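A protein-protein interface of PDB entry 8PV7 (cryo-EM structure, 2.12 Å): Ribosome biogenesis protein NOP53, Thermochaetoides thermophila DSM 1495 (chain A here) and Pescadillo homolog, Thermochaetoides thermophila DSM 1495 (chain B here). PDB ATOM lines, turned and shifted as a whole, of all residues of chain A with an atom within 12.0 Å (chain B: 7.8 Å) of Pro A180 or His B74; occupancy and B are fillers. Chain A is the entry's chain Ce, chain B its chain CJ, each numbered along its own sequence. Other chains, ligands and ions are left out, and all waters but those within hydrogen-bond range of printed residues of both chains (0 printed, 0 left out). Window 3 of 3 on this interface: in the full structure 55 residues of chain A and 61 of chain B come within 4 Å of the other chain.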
ATOM      1  N   PRO A 180      28.956  25.932  23.209  1.00  0.00           N
ATOM      2  CA  PRO A 180      28.394  26.600  22.030  1.00  0.00           C
ATOM      3  C   PRO A 180      28.394  25.702  20.795  1.00  0.00           C
ATOM      4  O   PRO A 180      29.450  25.291  20.316  1.00  0.00           O
ATOM      5  CB  PRO A 180      29.311  27.811  21.837  1.00  0.00           C
ATOM      6  CG  PRO A 180      30.596  27.435  22.493  1.00  0.00           C
ATOM      7  CD  PRO A 180      30.258  26.496  23.610  1.00  0.00           C
ATOM      8  N   ASP A 181      27.201  25.392  20.297  1.00  0.00           N
ATOM      9  CA  ASP A 181      27.075  24.505  19.153  1.00  0.00           C
ATOM     10  C   ASP A 181      27.406  25.240  17.854  1.00  0.00           C
ATOM     11  O   ASP A 181      27.080  26.419  17.694  1.00  0.00           O
ATOM     12  CB  ASP A 181      25.664  23.929  19.080  1.00  0.00           C
ATOM     13  CG  ASP A 181      25.525  22.636  19.855  1.00  0.00           C
ATOM     14  OD1 ASP A 181      26.198  22.490  20.895  1.00  0.00           O
ATOM     15  OD2 ASP A 181      24.750  21.759  19.420  1.00  0.00           O
ATOM     16  N   PRO A 182      28.064  24.563  16.909  1.00  0.00           N
ATOM     17  CA  PRO A 182      28.324  25.133  15.579  1.00  0.00           C
ATOM     18  C   PRO A 182      27.122  24.943  14.655  1.00  0.00           C
ATOM     19  O   PRO A 182      26.984  23.948  13.939  1.00  0.00           O
ATOM     20  CB  PRO A 182      29.549  24.348  15.107  1.00  0.00           C
ATOM     21  CG  PRO A 182      29.503  23.051  15.867  1.00  0.00           C
ATOM     22  CD  PRO A 182      28.488  23.159  16.969  1.00  0.00           C
ATOM     23  N   LEU A 183      26.204  25.912  14.698  1.00  0.00           N
ATOM     24  CA  LEU A 183      25.011  25.848  13.857  1.00  0.00           C
ATOM     25  C   LEU A 183      25.346  25.915  12.371  1.00  0.00           C
ATOM     26  O   LEU A 183      24.518  25.543  11.532  1.00  0.00           O
ATOM     27  CB  LEU A 183      24.034  26.968  14.229  1.00  0.00           C
ATOM     28  CG  LEU A 183      22.987  26.675  15.310  1.00  0.00           C
ATOM     29  CD1 LEU A 183      23.607  26.556  16.696  1.00  0.00           C
ATOM     30  CD2 LEU A 183      21.896  27.736  15.299  1.00  0.00           C
ATOM     31  N   LYS A 184      26.541  26.385  12.022  1.00  0.00           N
ATOM     32  CA  LYS A 184      27.042  26.276  10.660  1.00  0.00           C
ATOM     33  C   LYS A 184      28.000  25.090  10.576  1.00  0.00           C
ATOM     34  O   LYS A 184      28.773  24.839  11.506  1.00  0.00           O
ATOM     35  CB  LYS A 184      27.705  27.582  10.212  1.00  0.00           C
ATOM     36  CG  LYS A 184      28.873  28.100  11.062  1.00  0.00           C
ATOM     37  CD  LYS A 184      30.235  27.612  10.569  1.00  0.00           C
ATOM     38  CE  LYS A 184      31.323  28.639  10.784  1.00  0.00           C
ATOM     39  NZ  LYS A 184      32.660  28.072  10.451  1.00  0.00           N
ATOM     40  N   LYS A 185      27.925  24.357   9.476  1.00  0.00           N
ATOM     41  CA  LYS A 185      28.877  23.290   9.228  1.00  0.00           C
ATOM     42  C   LYS A 185      30.235  23.889   8.870  1.00  0.00           C
ATOM     43  O   LYS A 185      30.299  24.991   8.316  1.00  0.00           O
ATOM     44  CB  LYS A 185      28.378  22.402   8.090  1.00  0.00           C
ATOM     45  CG  LYS A 185      27.058  21.723   8.388  1.00  0.00           C
ATOM     46  CD  LYS A 185      26.505  21.016   7.165  1.00  0.00           C
ATOM     47  CE  LYS A 185      27.489  20.010   6.609  1.00  0.00           C
ATOM     48  NZ  LYS A 185      26.917  19.276   5.451  1.00  0.00           N
ATOM     49  N   PRO A 186      31.335  23.208   9.186  1.00  0.00           N
ATOM     50  CA  PRO A 186      32.646  23.678   8.725  1.00  0.00           C
ATOM     51  C   PRO A 186      32.792  23.520   7.217  1.00  0.00           C
ATOM     52  O   PRO A 186      32.077  22.745   6.580  1.00  0.00           O
ATOM     53  CB  PRO A 186      33.633  22.779   9.480  1.00  0.00           C
ATOM     54  CG  PRO A 186      32.845  22.198  10.616  1.00  0.00           C
ATOM     55  CD  PRO A 186      31.448  22.075  10.117  1.00  0.00           C
ATOM     56  N   THR A 188      35.357  22.236   5.869  1.00  0.00           N
ATOM     57  CA  THR A 188      35.941  20.916   5.673  1.00  0.00           C
ATOM     58  C   THR A 188      34.865  19.881   5.374  1.00  0.00           C
ATOM     59  O   THR A 188      35.103  18.927   4.627  1.00  0.00           O
ATOM     60  CB  THR A 188      36.749  20.523   6.905  1.00  0.00           C
ATOM     61  OG1 THR A 188      35.985  20.790   8.085  1.00  0.00           O
ATOM     62  CG2 THR A 188      38.048  21.304   6.955  1.00  0.00           C
ATOM     63  N   LEU A 189      33.672  20.059   5.941  1.00  0.00           N
ATOM     64  CA  LEU A 189      32.543  19.213   5.585  1.00  0.00           C
ATOM     65  C   LEU A 189      32.003  19.526   4.201  1.00  0.00           C
ATOM     66  O   LEU A 189      31.403  18.649   3.570  1.00  0.00           O
ATOM     67  CB  LEU A 189      31.428  19.357   6.614  1.00  0.00           C
ATOM     68  CG  LEU A 189      31.534  18.466   7.847  1.00  0.00           C
ATOM     69  CD1 LEU A 189      30.317  18.664   8.712  1.00  0.00           C
ATOM     70  CD2 LEU A 189      31.681  17.013   7.444  1.00  0.00           C
ATOM     71  N   LEU B  26      36.825  11.716  20.847  1.00  0.00           N
ATOM     72  CA  LEU B  26      35.385  11.667  21.037  1.00  0.00           C
ATOM     73  C   LEU B  26      34.964  10.751  22.179  1.00  0.00           C
ATOM     74  O   LEU B  26      33.800  10.804  22.584  1.00  0.00           O
ATOM     75  CB  LEU B  26      34.695  11.235  19.741  1.00  0.00           C
ATOM     76  CG  LEU B  26      34.815  12.207  18.566  1.00  0.00           C
ATOM     77  CD1 LEU B  26      34.239  11.597  17.315  1.00  0.00           C
ATOM     78  CD2 LEU B  26      34.133  13.522  18.878  1.00  0.00           C
ATOM     79  N   LYS B  40      26.940  11.134   9.679  1.00  0.00           N
ATOM     80  CA  LYS B  40      27.201  12.560   9.559  1.00  0.00           C
ATOM     81  C   LYS B  40      28.047  12.915   8.346  1.00  0.00           C
ATOM     82  O   LYS B  40      28.323  14.096   8.131  1.00  0.00           O
ATOM     83  CB  LYS B  40      27.877  13.089  10.828  1.00  0.00           C
ATOM     84  CG  LYS B  40      27.043  12.936  12.083  1.00  0.00           C
ATOM     85  CD  LYS B  40      26.156  14.136  12.331  1.00  0.00           C
ATOM     86  CE  LYS B  40      26.965  15.361  12.697  1.00  0.00           C
ATOM     87  NZ  LYS B  40      26.095  16.476  13.152  1.00  0.00           N
ATOM     88  N   LYS B  67      38.767  19.709  12.199  1.00  0.00           N
ATOM     89  CA  LYS B  67      37.537  20.482  12.311  1.00  0.00           C
ATOM     90  C   LYS B  67      36.296  19.605  12.199  1.00  0.00           C
ATOM     91  O   LYS B  67      35.298  19.869  12.874  1.00  0.00           O
ATOM     92  CB  LYS B  67      37.508  21.575  11.247  1.00  0.00           C
ATOM     93  CG  LYS B  67      37.823  22.960  11.768  1.00  0.00           C
ATOM     94  CD  LYS B  67      39.126  23.000  12.537  1.00  0.00           C
ATOM     95  CE  LYS B  67      39.271  24.305  13.292  1.00  0.00           C
ATOM     96  NZ  LYS B  67      39.103  25.475  12.390  1.00  0.00           N
ATOM     97  N   ASP B  68      36.341  18.555  11.374  1.00  0.00           N
ATOM     98  CA  ASP B  68      35.224  17.617  11.299  1.00  0.00           C
ATOM     99  C   ASP B  68      35.042  16.858  12.609  1.00  0.00           C
ATOM    100  O   ASP B  68      33.907  16.632  13.052  1.00  0.00           O
ATOM    101  CB  ASP B  68      35.431  16.642  10.144  1.00  0.00           C
ATOM    102  CG  ASP B  68      35.254  17.295   8.794  1.00  0.00           C
ATOM    103  OD1 ASP B  68      34.773  18.443   8.748  1.00  0.00           O
ATOM    104  OD2 ASP B  68      35.592  16.660   7.777  1.00  0.00           O
ATOM    105  N   ILE B  69      36.146  16.466  13.252  1.00  0.00           N
ATOM    106  CA  ILE B  69      36.039  15.799  14.551  1.00  0.00           C
ATOM    107  C   ILE B  69      35.506  16.763  15.615  1.00  0.00           C
ATOM    108  O   ILE B  69      34.670  16.392  16.457  1.00  0.00           O
ATOM    109  CB  ILE B  69      37.401  15.190  14.943  1.00  0.00           C
ATOM    110  CG1 ILE B  69      37.922  14.268  13.838  1.00  0.00           C
ATOM    111  CG2 ILE B  69      37.322  14.446  16.264  1.00  0.00           C
ATOM    112  CD1 ILE B  69      36.967  13.179  13.437  1.00  0.00           C
ATOM    113  N   GLN B  70      35.967  18.015  15.578  1.00  0.00           N
ATOM    114  CA  GLN B  70      35.451  19.049  16.473  1.00  0.00           C
ATOM    115  C   GLN B  70      33.958  19.261  16.277  1.00  0.00           C
ATOM    116  O   GLN B  70      33.226  19.499  17.241  1.00  0.00           O
ATOM    117  CB  GLN B  70      36.189  20.364  16.237  1.00  0.00           C
ATOM    118  CG  GLN B  70      37.641  20.358  16.616  1.00  0.00           C
ATOM    119  CD  GLN B  70      37.881  20.957  17.963  1.00  0.00           C
ATOM    120  OE1 GLN B  70      36.941  21.324  18.665  1.00  0.00           O
ATOM    121  NE2 GLN B  70      39.147  21.082  18.334  1.00  0.00           N
ATOM    122  N   TYR B  71      33.499  19.204  15.029  1.00  0.00           N
ATOM    123  CA  TYR B  71      32.073  19.301  14.750  1.00  0.00           C
ATOM    124  C   TYR B  71      31.313  18.110  15.321  1.00  0.00           C
ATOM    125  O   TYR B  71      30.219  18.271  15.871  1.00  0.00           O
ATOM    126  CB  TYR B  71      31.854  19.412  13.245  1.00  0.00           C
ATOM    127  CG  TYR B  71      30.411  19.523  12.844  1.00  0.00           C
ATOM    128  CD1 TYR B  71      29.698  20.688  13.067  1.00  0.00           C
ATOM    129  CD2 TYR B  71      29.763  18.466  12.230  1.00  0.00           C
ATOM    130  CE1 TYR B  71      28.382  20.796  12.694  1.00  0.00           C
ATOM    131  CE2 TYR B  71      28.448  18.564  11.851  1.00  0.00           C
ATOM    132  CZ  TYR B  71      27.762  19.730  12.086  1.00  0.00           C
ATOM    133  OH  TYR B  71      26.447  19.831  11.713  1.00  0.00           O
ATOM    134  N   LEU B  72      31.889  16.907  15.212  1.00  0.00           N
ATOM    135  CA  LEU B  72      31.252  15.719  15.783  1.00  0.00           C
ATOM    136  C   LEU B  72      31.154  15.780  17.301  1.00  0.00           C
ATOM    137  O   LEU B  72      30.335  15.069  17.889  1.00  0.00           O
ATOM    138  CB  LEU B  72      32.004  14.455  15.383  1.00  0.00           C
ATOM    139  CG  LEU B  72      31.767  13.904  13.987  1.00  0.00           C
ATOM    140  CD1 LEU B  72      32.571  12.635  13.811  1.00  0.00           C
ATOM    141  CD2 LEU B  72      30.296  13.645  13.786  1.00  0.00           C
ATOM    142  N   LEU B  73      31.996  16.589  17.950  1.00  0.00           N
ATOM    143  CA  LEU B  73      31.893  16.750  19.403  1.00  0.00           C
ATOM    144  C   LEU B  73      30.537  17.281  19.871  1.00  0.00           C
ATOM    145  O   LEU B  73      30.165  17.045  21.023  1.00  0.00           O
ATOM    146  CB  LEU B  73      32.973  17.690  19.929  1.00  0.00           C
ATOM    147  CG  LEU B  73      34.360  17.129  20.202  1.00  0.00           C
ATOM    148  CD1 LEU B  73      35.360  18.262  20.270  1.00  0.00           C
ATOM    149  CD2 LEU B  73      34.353  16.327  21.488  1.00  0.00           C
ATOM    150  N   HIS B  74      29.788  17.981  19.024  1.00  0.00           N
ATOM    151  CA  HIS B  74      28.544  18.613  19.441  1.00  0.00           C
ATOM    152  C   HIS B  74      27.290  17.849  19.031  1.00  0.00           C
ATOM    153  O   HIS B  74      26.185  18.356  19.237  1.00  0.00           O
ATOM    154  CB  HIS B  74      28.471  20.031  18.879  1.00  0.00           C
ATOM    155  CG  HIS B  74      29.587  20.913  19.332  1.00  0.00           C
ATOM    156  ND1 HIS B  74      29.548  21.607  20.519  1.00  0.00           N
ATOM    157  CD2 HIS B  74      30.764  21.233  18.747  1.00  0.00           C
ATOM    158  CE1 HIS B  74      30.660  22.305  20.655  1.00  0.00           C
ATOM    159  NE2 HIS B  74      31.414  22.095  19.591  1.00  0.00           N
ATOM    160  N   GLU B  75      27.427  16.657  18.474  1.00  0.00           N
ATOM    161  CA  GLU B  75      26.270  15.924  17.972  1.00  0.00           C
ATOM    162  C   GLU B  75      25.460  15.337  19.125  1.00  0.00           C
ATOM    163  O   GLU B  75      26.027  14.682  20.004  1.00  0.00           O
ATOM    164  CB  GLU B  75      26.726  14.825  17.014  1.00  0.00           C
ATOM    165  CG  GLU B  75      25.684  13.768  16.717  1.00  0.00           C
ATOM    166  CD  GLU B  75      24.479  14.314  15.985  1.00  0.00           C
ATOM    167  OE1 GLU B  75      24.647  15.202  15.125  1.00  0.00           O
ATOM    168  OE2 GLU B  75      23.358  13.862  16.282  1.00  0.00           O
ATOM    169  N   PRO B  76      24.142  15.559  19.164  1.00  0.00           N
ATOM    170  CA  PRO B  76      23.329  15.033  20.276  1.00  0.00           C
ATOM    171  C   PRO B  76      23.222  13.515  20.342  1.00  0.00           C
ATOM    172  O   PRO B  76      22.695  12.997  21.332  1.00  0.00           O
ATOM    173  CB  PRO B  76      21.956  15.668  20.024  1.00  0.00           C
ATOM    174  CG  PRO B  76      22.250  16.895  19.264  1.00  0.00           C
ATOM    175  CD  PRO B  76      23.407  16.565  18.381  1.00  0.00           C
ATOM    176  N   LEU B  77      23.682  12.783  19.326  1.00  0.00           N
ATOM    177  CA  LEU B  77      23.601  11.327  19.373  1.00  0.00           C
ATOM    178  C   LEU B  77      24.583  10.723  20.367  1.00  0.00           C
ATOM    179  O   LEU B  77      24.414   9.569  20.768  1.00  0.00           O
ATOM    180  CB  LEU B  77      23.848  10.738  17.988  1.00  0.00           C
ATOM    181  CG  LEU B  77      22.647  10.638  17.056  1.00  0.00           C
ATOM    182  CD1 LEU B  77      23.104  10.149  15.711  1.00  0.00           C
ATOM    183  CD2 LEU B  77      21.594   9.713  17.628  1.00  0.00           C
ATOM    184  N   LEU B  78      25.618  11.470  20.759  1.00  0.00           N
ATOM    185  CA  LEU B  78      26.590  10.962  21.726  1.00  0.00           C
ATOM    186  C   LEU B  78      25.942  10.703  23.081  1.00  0.00           C
ATOM    187  O   LEU B  78      26.162   9.655  23.709  1.00  0.00           O
ATOM    188  CB  LEU B  78      27.744  11.953  21.863  1.00  0.00           C
ATOM    189  CG  LEU B  78      28.585  12.187  20.611  1.00  0.00           C
ATOM    190  CD1 LEU B  78      29.708  13.148  20.907  1.00  0.00           C
ATOM    191  CD2 LEU B  78      29.138  10.875  20.114  1.00  0.00           C
ATOM    192  N   HIS B 125      17.096  14.778  12.898  1.00  0.00           N
ATOM    193  CA  HIS B 125      17.879  16.008  12.886  1.00  0.00           C
ATOM    194  C   HIS B 125      19.069  15.895  11.942  1.00  0.00           C
ATOM    195  O   HIS B 125      19.530  16.899  11.389  1.00  0.00           O
ATOM    196  CB  HIS B 125      18.351  16.339  14.299  1.00  0.00           C
ATOM    197  CG  HIS B 125      19.270  15.313  14.884  1.00  0.00           C
ATOM    198  ND1 HIS B 125      18.837  14.071  15.297  1.00  0.00           N
ATOM    199  CD2 HIS B 125      20.605  15.338  15.107  1.00  0.00           C
ATOM    200  CE1 HIS B 125      19.864  13.381  15.757  1.00  0.00           C
ATOM    201  NE2 HIS B 125      20.948  14.126  15.653  1.00  0.00           N
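The side-chain carboxylate of Asp A181 lies within hydrogen-bond range of a ring nitrogen (ND1) of His B74 (3.5 Å).
OG1 of Thr A188 is in hydrogen-bond range of OD1 of Asp B68 (2.7 Å).
The backbone NH (N) of Leu A189 lies close to the side-chain carboxylate (OD1) of Asp B68.
Among the printed residues, pairs that only touch across the chains: Pro A180 with His B74 (3.2 Å), Pro A182 with Tyr B71 (3.7 Å), Pro A182 with His B74 (3.4 Å), Lys A185 with Tyr B71 (3.9 Å), Pro A186 with Tyr B71 (3.7 Å), Thr A188 with Lys B67 (3.6 Å) and Leu A189 with Tyr B71 (3.6 Å).
Pro A180 touches one residue of chain B.
Leu A183 touches none of the printed residues of chain B.
Of the printed residues of chain B, Leu A189 touches Asp B68 and Tyr B71.
Printed residues of chain A within 4 Å of Lys B67: Thr A188.
Tyr B71 touches just these residues of chain A: Pro A182, Lys A185, Pro A186 and Leu A189.
No residue of chain A comes within 4 Å of Leu B73.
Of chain A, only Pro A180 (3.2 Å), Asp A181 (3.5 Å) and Pro A182 (3.4 Å) come within 4 Å of His B74.
No residue of chain A comes within 4 Å of Glu B75.
No residue of chain A comes within 4 Å of Pro B76.
The nearest residue of chain B that does not touch Pro A180 is Gln B70 (7.6 Å).
Of the 15 printed residues of chain B, 4 touch a printed residue of chain A.
Of the 9 printed residues of chain A, 7 touch a printed residue of chain B.
Among the printed residues, no Asp or Glu carboxylate lies within 4 Å of a Lys or Arg side-chain nitrogen of the other chain.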
